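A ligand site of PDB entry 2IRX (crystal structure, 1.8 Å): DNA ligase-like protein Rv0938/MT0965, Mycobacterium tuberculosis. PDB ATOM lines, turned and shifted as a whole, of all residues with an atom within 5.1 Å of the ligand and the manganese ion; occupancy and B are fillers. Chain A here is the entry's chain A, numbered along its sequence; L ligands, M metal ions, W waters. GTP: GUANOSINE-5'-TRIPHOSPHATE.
Residues that only touch the ligand: Phe 67 (3.3 Å), Gln 233 (3.4 Å) and Thr 240 (3.8 Å).
Of the 20 residues printed, 15 come within 4 Å of the ligand.
The nearest printed residue that does not touch the ligand is Ile 241 (4.1 Å).
OD1 of Asp 142 is bound to the manganese ion, at 2.2 Å.
Water W11 is bound to the manganese ion (2.2 Å).
OD1 of Asp 140 binds the manganese ion, 2.2 Å away.
The manganese ion is bound by O2G of the ligand (2.2 Å).
The manganese ion is bound by an oxygen (O1B) of the ligand (2.3 Å).
The manganese ion is bound by water W12 (2.5 Å).
The manganese ion has six donor atoms within binding distance.
Merely in contact with the manganese ion: His 181 (3.997 Å).
Of the 20 residues printed, 3 come within 4 Å of the manganese ion.
The nearest printed residue that does not touch the manganese ion is Leu 141 (4.4 Å).
Water W12 lies within hydrogen-bond range of an oxygen (O1G) of the ligand (2.8 Å), the backbone carbonyl oxygen (O) of Leu 141 (2.9 Å), the backbone NH (N) of Leu 180 (3.4 Å) and a ring nitrogen (NE2) of His 181 (3.5 Å).
Water W7 bridges NH2 of Arg 249 (2.6 Å) and O2A of the ligand (2.8 Å).
Water W1 bridges an oxygen (O2B) of the ligand (2.9 Å) and the backbone NH of Ile 241 (2.9 Å).
Water W10 lies within hydrogen-bond range of OE1 of Gln 233 (2.7 Å), OD2 of Asp 140 (2.8 Å) and NE2 of His 181 (3.5 Å).
Water W9 lies within hydrogen-bond range of an oxygen (O3') of the ligand (3.0 Å) and the backbone NH (N) of Thr 239 (3.1 Å).
Water W14 bridges the side-chain amino group of Lys 69 (2.8 Å) and a nitrogen (N2) of the ligand (3.1 Å).
OG of Ser 177 sits at hydrogen-bond distance from NE of Arg 249, at 3.0 Å.
A ring nitrogen (ND1) of His 114 lies within hydrogen-bond range of the backbone NH (N) of Ile 241 (3.4 Å).
OD2 of Asp 140 sits at hydrogen-bond distance from NE2 of Gln 233, 2.6 Å away.
The side-chain hydroxyl (OG) of Ser 175 lies within hydrogen-bond range of the backbone carbonyl oxygen (O) of Gly 179 (3.4 Å).
The side-chain carboxylate (OD1) of Asp 140 lies close to a ring nitrogen (NE2) of His 181.
O of Thr 239 lies close to OE1 of Gln 233 (3.5 Å).
The backbone NH (N) of Lys 55 sits at hydrogen-bond distance from the backbone carbonyl oxygen (O) of Glu 112 (2.9 Å).
The side-chain carboxylate of Glu 112 lies within salt-bridge range of the guanidinium group of Arg 247, at 2.9 Å.
A nitrogen (N7) of the ligand lies within hydrogen-bond range of the side-chain amino group of Lys 55.
An oxygen (O2') of the ligand sits at hydrogen-bond distance from the side-chain hydroxyl of Thr 239, 2.7 Å away.
The backbone NH (N) of Gly 179 is in hydrogen-bond range of an oxygen (O1G) of the ligand (3.0 Å).
O1A of the ligand lies within salt-bridge range of NH2 of Arg 249 (3.4 Å).
A ring nitrogen (NE2) of His 181 lies close to an oxygen (O1B) of the ligand, 2.8 Å away.
OG of Ser 177 sits at hydrogen-bond distance from O3G of the ligand (2.5 Å).
An oxygen (O2') of the ligand sits at hydrogen-bond distance from a ring nitrogen (ND1) of His 114, 2.9 Å away.
An oxygen (O3G) of the ligand is in salt-bridge range of the side-chain amino group (NZ) of Lys 178 (3.0 Å).
The side-chain hydroxyl (OG) of Ser 175 lies within hydrogen-bond range of an oxygen (O1G) of the ligand.
N of Lys 178 lies within hydrogen-bond range of O1G of the ligand.
An oxygen (O2B) of the ligand lies within salt-bridge range of the guanidinium group (NH2) of Arg 247 (2.7 Å).
The backbone carbonyl oxygen of Thr 239 lies within hydrogen-bond range of an oxygen (O3') of the ligand (2.6 Å).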
ATOM      1  N   LYS A  55     -30.022  10.858 -11.448  1.00  0.00           N
ATOM      2  CA  LYS A  55     -30.062  11.581 -12.719  1.00  0.00           C
ATOM      3  C   LYS A  55     -31.517  11.982 -13.037  1.00  0.00           C
ATOM      4  O   LYS A  55     -32.392  11.119 -13.316  1.00  0.00           O
ATOM      5  CB  LYS A  55     -29.411  10.783 -13.844  1.00  0.00           C
ATOM      6  CG  LYS A  55     -28.965  11.644 -15.028  1.00  0.00           C
ATOM      7  CD  LYS A  55     -28.057  10.862 -15.989  1.00  0.00           C
ATOM      8  CE  LYS A  55     -27.709  11.731 -17.221  1.00  0.00           C
ATOM      9  NZ  LYS A  55     -26.718  11.017 -18.151  1.00  0.00           N
ATOM     10  N   PHE A  67     -27.009  15.376 -13.066  1.00  0.00           N
ATOM     11  CA  PHE A  67     -26.579  14.242 -12.284  1.00  0.00           C
ATOM     12  C   PHE A  67     -26.454  14.787 -10.862  1.00  0.00           C
ATOM     13  O   PHE A  67     -25.453  15.469 -10.513  1.00  0.00           O
ATOM     14  CB  PHE A  67     -25.250  13.787 -12.866  1.00  0.00           C
ATOM     15  CG  PHE A  67     -24.847  12.379 -12.546  1.00  0.00           C
ATOM     16  CD1 PHE A  67     -25.635  11.290 -12.952  1.00  0.00           C
ATOM     17  CD2 PHE A  67     -23.628  12.143 -11.889  1.00  0.00           C
ATOM     18  CE1 PHE A  67     -25.240   9.957 -12.681  1.00  0.00           C
ATOM     19  CE2 PHE A  67     -23.197  10.817 -11.638  1.00  0.00           C
ATOM     20  CZ  PHE A  67     -24.007   9.723 -12.023  1.00  0.00           C
ATOM     21  N   LYS A  69     -25.958  14.710  -6.950  1.00  0.00           N
ATOM     22  CA  LYS A  69     -25.319  13.913  -5.896  1.00  0.00           C
ATOM     23  C   LYS A  69     -25.716  14.431  -4.527  1.00  0.00           C
ATOM     24  O   LYS A  69     -26.383  13.726  -3.751  1.00  0.00           O
ATOM     25  CB  LYS A  69     -23.793  13.936  -6.064  1.00  0.00           C
ATOM     26  CG  LYS A  69     -23.276  13.302  -7.389  1.00  0.00           C
ATOM     27  CD  LYS A  69     -21.759  13.456  -7.526  1.00  0.00           C
ATOM     28  CE  LYS A  69     -21.300  12.901  -8.893  1.00  0.00           C
ATOM     29  NZ  LYS A  69     -19.812  13.140  -9.124  1.00  0.00           N
ATOM     30  N   GLU A 112     -33.155   7.908 -13.493  1.00  0.00           N
ATOM     31  CA  GLU A 112     -32.056   6.971 -13.265  1.00  0.00           C
ATOM     32  C   GLU A 112     -31.499   7.105 -11.856  1.00  0.00           C
ATOM     33  O   GLU A 112     -31.280   8.224 -11.345  1.00  0.00           O
ATOM     34  CB  GLU A 112     -30.919   7.176 -14.299  1.00  0.00           C
ATOM     35  CG  GLU A 112     -31.394   7.148 -15.758  1.00  0.00           C
ATOM     36  CD  GLU A 112     -30.279   7.115 -16.769  1.00  0.00           C
ATOM     37  OE1 GLU A 112     -29.116   7.370 -16.384  1.00  0.00           O
ATOM     38  OE2 GLU A 112     -30.553   6.815 -17.958  1.00  0.00           O
ATOM     39  N   HIS A 114     -28.213   5.900  -9.831  1.00  0.00           N
ATOM     40  CA  HIS A 114     -26.827   5.413  -9.990  1.00  0.00           C
ATOM     41  C   HIS A 114     -26.175   5.164  -8.611  1.00  0.00           C
ATOM     42  O   HIS A 114     -26.338   5.978  -7.699  1.00  0.00           O
ATOM     43  CB  HIS A 114     -26.004   6.384 -10.830  1.00  0.00           C
ATOM     44  CG  HIS A 114     -26.470   6.512 -12.253  1.00  0.00           C
ATOM     45  ND1 HIS A 114     -25.722   6.087 -13.326  1.00  0.00           N
ATOM     46  CD2 HIS A 114     -27.613   7.037 -12.778  1.00  0.00           C
ATOM     47  CE1 HIS A 114     -26.374   6.333 -14.448  1.00  0.00           C
ATOM     48  NE2 HIS A 114     -27.523   6.901 -14.150  1.00  0.00           N
ATOM     49  N   ASP A 140     -18.741  -2.601 -17.453  1.00  0.00           N
ATOM     50  CA  ASP A 140     -19.587  -1.793 -18.306  1.00  0.00           C
ATOM     51  C   ASP A 140     -19.096  -2.049 -19.751  1.00  0.00           C
ATOM     52  O   ASP A 140     -18.009  -1.629 -20.139  1.00  0.00           O
ATOM     53  CB  ASP A 140     -19.463  -0.320 -17.861  1.00  0.00           C
ATOM     54  CG  ASP A 140     -20.276   0.642 -18.727  1.00  0.00           C
ATOM     55  OD1 ASP A 140     -21.069   0.190 -19.580  1.00  0.00           O
ATOM     56  OD2 ASP A 140     -20.133   1.889 -18.558  1.00  0.00           O
ATOM     57  N   LEU A 141     -19.904  -2.761 -20.524  1.00  0.00           N
ATOM     58  CA  LEU A 141     -19.510  -3.120 -21.899  1.00  0.00           C
ATOM     59  C   LEU A 141     -20.196  -2.183 -22.896  1.00  0.00           C
ATOM     60  O   LEU A 141     -21.435  -2.209 -23.021  1.00  0.00           O
ATOM     61  CB  LEU A 141     -19.895  -4.579 -22.228  1.00  0.00           C
ATOM     62  CG  LEU A 141     -18.963  -5.731 -21.784  1.00  0.00           C
ATOM     63  CD1 LEU A 141     -18.664  -5.721 -20.289  1.00  0.00           C
ATOM     64  CD2 LEU A 141     -19.528  -7.086 -22.209  1.00  0.00           C
ATOM     65  N   ASP A 142     -19.374  -1.413 -23.627  1.00  0.00           N
ATOM     66  CA  ASP A 142     -19.828  -0.445 -24.629  1.00  0.00           C
ATOM     67  C   ASP A 142     -19.451  -0.890 -26.047  1.00  0.00           C
ATOM     68  O   ASP A 142     -18.287  -1.100 -26.324  1.00  0.00           O
ATOM     69  CB  ASP A 142     -19.150   0.902 -24.381  1.00  0.00           C
ATOM     70  CG  ASP A 142     -19.631   1.551 -23.099  1.00  0.00           C
ATOM     71  OD1 ASP A 142     -20.647   1.096 -22.586  1.00  0.00           O
ATOM     72  OD2 ASP A 142     -18.977   2.492 -22.614  1.00  0.00           O
ATOM     73  N   SER A 175     -28.217  -2.893 -20.386  1.00  0.00           N
ATOM     74  CA  SER A 175     -28.166  -1.590 -19.700  1.00  0.00           C
ATOM     75  C   SER A 175     -29.417  -0.716 -19.819  1.00  0.00           C
ATOM     76  O   SER A 175     -29.622   0.190 -19.024  1.00  0.00           O
ATOM     77  CB  SER A 175     -26.974  -0.754 -20.200  1.00  0.00           C
ATOM     78  OG  SER A 175     -27.271  -0.269 -21.492  1.00  0.00           O
ATOM     79  N   SER A 177     -29.752   1.005 -22.553  1.00  0.00           N
ATOM     80  CA  SER A 177     -29.280   2.012 -23.482  1.00  0.00           C
ATOM     81  C   SER A 177     -28.644   1.302 -24.690  1.00  0.00           C
ATOM     82  O   SER A 177     -29.373   0.860 -25.563  1.00  0.00           O
ATOM     83  CB  SER A 177     -28.345   2.987 -22.763  1.00  0.00           C
ATOM     84  OG  SER A 177     -27.839   4.002 -23.641  1.00  0.00           O
ATOM     85  N   LYS A 178     -27.335   1.136 -24.723  1.00  0.00           N
ATOM     86  CA  LYS A 178     -26.660   0.581 -25.914  1.00  0.00           C
ATOM     87  C   LYS A 178     -25.942  -0.763 -25.684  1.00  0.00           C
ATOM     88  O   LYS A 178     -25.665  -1.509 -26.636  1.00  0.00           O
ATOM     89  CB  LYS A 178     -25.646   1.607 -26.457  1.00  0.00           C
ATOM     90  CG  LYS A 178     -26.315   2.773 -27.208  1.00  0.00           C
ATOM     91  CD  LYS A 178     -25.483   4.060 -27.370  1.00  0.00           C
ATOM     92  CE  LYS A 178     -23.993   3.960 -27.028  1.00  0.00           C
ATOM     93  NZ  LYS A 178     -23.726   4.511 -25.641  1.00  0.00           N
ATOM     94  N   GLY A 179     -25.604  -1.037 -24.419  1.00  0.00           N
ATOM     95  CA  GLY A 179     -24.708  -2.155 -24.088  1.00  0.00           C
ATOM     96  C   GLY A 179     -25.201  -3.089 -23.002  1.00  0.00           C
ATOM     97  O   GLY A 179     -26.399  -3.299 -22.814  1.00  0.00           O
ATOM     98  N   LEU A 180     -24.235  -3.669 -22.289  1.00  0.00           N
ATOM     99  CA  LEU A 180     -24.494  -4.692 -21.283  1.00  0.00           C
ATOM    100  C   LEU A 180     -23.700  -4.352 -20.043  1.00  0.00           C
ATOM    101  O   LEU A 180     -22.591  -3.818 -20.148  1.00  0.00           O
ATOM    102  CB  LEU A 180     -24.030  -6.066 -21.770  1.00  0.00           C
ATOM    103  CG  LEU A 180     -24.656  -6.767 -22.947  1.00  0.00           C
ATOM    104  CD1 LEU A 180     -23.912  -8.084 -23.226  1.00  0.00           C
ATOM    105  CD2 LEU A 180     -26.134  -7.053 -22.643  1.00  0.00           C
ATOM    106  N   HIS A 181     -24.254  -4.647 -18.884  1.00  0.00           N
ATOM    107  CA  HIS A 181     -23.518  -4.545 -17.633  1.00  0.00           C
ATOM    108  C   HIS A 181     -23.427  -5.961 -17.051  1.00  0.00           C
ATOM    109  O   HIS A 181     -24.372  -6.751 -17.176  1.00  0.00           O
ATOM    110  CB  HIS A 181     -24.239  -3.599 -16.650  1.00  0.00           C
ATOM    111  CG  HIS A 181     -24.292  -2.165 -17.111  1.00  0.00           C
ATOM    112  ND1 HIS A 181     -25.114  -1.233 -16.510  1.00  0.00           N
ATOM    113  CD2 HIS A 181     -23.634  -1.516 -18.090  1.00  0.00           C
ATOM    114  CE1 HIS A 181     -24.941  -0.059 -17.093  1.00  0.00           C
ATOM    115  NE2 HIS A 181     -24.063  -0.207 -18.079  1.00  0.00           N
ATOM    116  N   GLN A 233     -15.338   1.504 -13.308  1.00  0.00           N
ATOM    117  CA  GLN A 233     -16.459   1.880 -12.450  1.00  0.00           C
ATOM    118  C   GLN A 233     -16.419   1.097 -11.155  1.00  0.00           C
ATOM    119  O   GLN A 233     -17.244   1.300 -10.270  1.00  0.00           O
ATOM    120  CB  GLN A 233     -17.807   1.766 -13.166  1.00  0.00           C
ATOM    121  CG  GLN A 233     -18.033   2.860 -14.175  1.00  0.00           C
ATOM    122  CD  GLN A 233     -19.020   2.483 -15.272  1.00  0.00           C
ATOM    123  OE1 GLN A 233     -20.109   1.979 -14.988  1.00  0.00           O
ATOM    124  NE2 GLN A 233     -18.668   2.768 -16.533  1.00  0.00           N
ATOM    125  N   THR A 239     -19.739   5.437 -10.212  1.00  0.00           N
ATOM    126  CA  THR A 239     -21.067   4.817 -10.058  1.00  0.00           C
ATOM    127  C   THR A 239     -21.394   4.012 -11.318  1.00  0.00           C
ATOM    128  O   THR A 239     -20.693   4.100 -12.307  1.00  0.00           O
ATOM    129  CB  THR A 239     -22.188   5.898  -9.827  1.00  0.00           C
ATOM    130  OG1 THR A 239     -22.183   6.855 -10.904  1.00  0.00           O
ATOM    131  CG2 THR A 239     -22.026   6.622  -8.465  1.00  0.00           C
ATOM    132  N   THR A 240     -22.450   3.207 -11.239  1.00  0.00           N
ATOM    133  CA  THR A 240     -23.051   2.530 -12.390  1.00  0.00           C
ATOM    134  C   THR A 240     -24.535   2.546 -12.105  1.00  0.00           C
ATOM    135  O   THR A 240     -24.970   2.390 -10.941  1.00  0.00           O
ATOM    136  CB  THR A 240     -22.528   1.063 -12.553  1.00  0.00           C
ATOM    137  OG1 THR A 240     -21.075   1.090 -12.675  1.00  0.00           O
ATOM    138  CG2 THR A 240     -23.145   0.416 -13.814  1.00  0.00           C
ATOM    139  N   ILE A 241     -25.336   2.705 -13.153  1.00  0.00           N
ATOM    140  CA  ILE A 241     -26.791   2.688 -12.993  1.00  0.00           C
ATOM    141  C   ILE A 241     -27.236   1.419 -12.227  1.00  0.00           C
ATOM    142  O   ILE A 241     -26.709   0.313 -12.475  1.00  0.00           O
ATOM    143  CB  ILE A 241     -27.532   2.832 -14.342  1.00  0.00           C
ATOM    144  CG1 ILE A 241     -28.991   3.265 -14.102  1.00  0.00           C
ATOM    145  CG2 ILE A 241     -27.432   1.502 -15.209  1.00  0.00           C
ATOM    146  CD1 ILE A 241     -29.679   3.735 -15.371  1.00  0.00           C
ATOM    147  N   ARG A 247     -34.330   4.192 -17.729  1.00  0.00           N
ATOM    148  CA  ARG A 247     -33.351   5.017 -18.454  1.00  0.00           C
ATOM    149  C   ARG A 247     -33.986   6.324 -18.938  1.00  0.00           C
ATOM    150  O   ARG A 247     -35.131   6.357 -19.379  1.00  0.00           O
ATOM    151  CB  ARG A 247     -32.819   4.293 -19.705  1.00  0.00           C
ATOM    152  CG  ARG A 247     -32.225   2.914 -19.443  1.00  0.00           C
ATOM    153  CD  ARG A 247     -31.122   2.910 -18.405  1.00  0.00           C
ATOM    154  NE  ARG A 247     -30.134   3.991 -18.489  1.00  0.00           N
ATOM    155  CZ  ARG A 247     -28.811   3.853 -18.600  1.00  0.00           C
ATOM    156  NH1 ARG A 247     -28.042   4.951 -18.577  1.00  0.00           N
ATOM    157  NH2 ARG A 247     -28.213   2.649 -18.708  1.00  0.00           N
ATOM    158  N   ARG A 249     -33.961   7.911 -21.785  1.00  0.00           N
ATOM    159  CA  ARG A 249     -33.717   7.754 -23.226  1.00  0.00           C
ATOM    160  C   ARG A 249     -35.085   7.918 -23.875  1.00  0.00           C
ATOM    161  O   ARG A 249     -36.079   8.084 -23.156  1.00  0.00           O
ATOM    162  CB  ARG A 249     -33.134   6.354 -23.536  1.00  0.00           C
ATOM    163  CG  ARG A 249     -31.816   5.995 -22.824  1.00  0.00           C
ATOM    164  CD  ARG A 249     -30.656   6.864 -23.354  1.00  0.00           C
ATOM    165  NE  ARG A 249     -29.337   6.480 -22.841  1.00  0.00           N
ATOM    166  CZ  ARG A 249     -28.783   6.895 -21.694  1.00  0.00           C
ATOM    167  NH1 ARG A 249     -29.443   7.712 -20.852  1.00  0.00           N
ATOM    168  NH2 ARG A 249     -27.566   6.450 -21.390  1.00  0.00           N
HETATM  169  PG  GTP L   1     -24.779   2.603 -22.384  1.00  0.00           P
HETATM  170  O1G GTP L   1     -25.254   1.201 -22.526  1.00  0.00           O
HETATM  171  O2G GTP L   1     -23.269   2.675 -22.431  1.00  0.00           O
HETATM  172  O3G GTP L   1     -25.428   3.526 -23.366  1.00  0.00           O
HETATM  173  O3B GTP L   1     -25.343   3.065 -20.930  1.00  0.00           O
HETATM  174  PB  GTP L   1     -24.573   3.204 -19.541  1.00  0.00           P
HETATM  175  O1B GTP L   1     -23.496   2.169 -19.374  1.00  0.00           O
HETATM  176  O2B GTP L   1     -25.545   3.087 -18.426  1.00  0.00           O
HETATM  177  O3A GTP L   1     -23.840   4.609 -19.716  1.00  0.00           O
HETATM  178  PA  GTP L   1     -24.090   6.062 -19.061  1.00  0.00           P
HETATM  179  O1A GTP L   1     -25.525   6.237 -18.626  1.00  0.00           O
HETATM  180  O2A GTP L   1     -23.631   7.027 -20.125  1.00  0.00           O
HETATM  181  O5' GTP L   1     -23.109   6.081 -17.808  1.00  0.00           O
HETATM  182  C5' GTP L   1     -21.699   5.856 -17.924  1.00  0.00           C
HETATM  183  C4' GTP L   1     -21.004   6.301 -16.622  1.00  0.00           C
HETATM  184  O4' GTP L   1     -21.242   7.667 -16.307  1.00  0.00           O
HETATM  185  C3' GTP L   1     -21.496   5.520 -15.418  1.00  0.00           C
HETATM  186  O3' GTP L   1     -20.389   5.467 -14.553  1.00  0.00           O
HETATM  187  C2' GTP L   1     -22.578   6.419 -14.804  1.00  0.00           C
HETATM  188  O2' GTP L   1     -22.877   6.270 -13.428  1.00  0.00           O
HETATM  189  C1' GTP L   1     -22.039   7.802 -15.107  1.00  0.00           C
HETATM  190  N9  GTP L   1     -22.988   8.844 -15.515  1.00  0.00           N
HETATM  191  C8  GTP L   1     -24.137   8.744 -16.265  1.00  0.00           C
HETATM  192  N7  GTP L   1     -24.610   9.987 -16.448  1.00  0.00           N
HETATM  193  C5  GTP L   1     -23.755  10.884 -15.869  1.00  0.00           C
HETATM  194  C6  GTP L   1     -23.747  12.280 -15.783  1.00  0.00           C
HETATM  195  O6  GTP L   1     -24.657  12.945 -16.287  1.00  0.00           O
HETATM  196  N1  GTP L   1     -22.692  12.909 -15.132  1.00  0.00           N
HETATM  197  C2  GTP L   1     -21.654  12.175 -14.574  1.00  0.00           C
HETATM  198  N2  GTP L   1     -20.671  12.810 -13.928  1.00  0.00           N
HETATM  199  N3  GTP L   1     -21.676  10.780 -14.651  1.00  0.00           N
HETATM  200  C4  GTP L   1     -22.719  10.166 -15.305  1.00  0.00           C
HETATM  201 MN    MN M   1     -21.999   1.620 -20.973  1.00  0.00          MN
HETATM  202  O   HOH W   1     -24.495   3.586 -15.780  1.00  0.00           O
HETATM  203  O   HOH W   2     -27.435   8.104 -18.416  1.00  0.00           O
HETATM  204  O   HOH W   3     -26.293  15.279 -16.850  1.00  0.00           O
HETATM  205  O   HOH W   4     -21.380  15.470 -12.541  1.00  0.00           O
HETATM  206  O   HOH W   5     -22.805  13.742 -18.839  1.00  0.00           O
HETATM  207  O   HOH W   6     -22.775  15.749 -14.987  1.00  0.00           O
HETATM  208  O   HOH W   7     -25.145   6.385 -22.362  1.00  0.00           O
HETATM  209  O   HOH W   8     -22.079   2.486 -24.985  1.00  0.00           O
HETATM  210  O   HOH W   9     -18.881   7.163 -12.583  1.00  0.00           O
HETATM  211  O   HOH W  10     -22.198   2.353 -16.692  1.00  0.00           O
HETATM  212  O   HOH W  11     -20.765   3.387 -20.721  1.00  0.00           O
HETATM  213  O   HOH W  12     -23.236  -0.503 -21.461  1.00  0.00           O
HETATM  214  O   HOH W  13     -21.618   6.078 -21.458  1.00  0.00           O
HETATM  215  O   HOH W  14     -18.915  11.997 -11.492  1.00  0.00           O
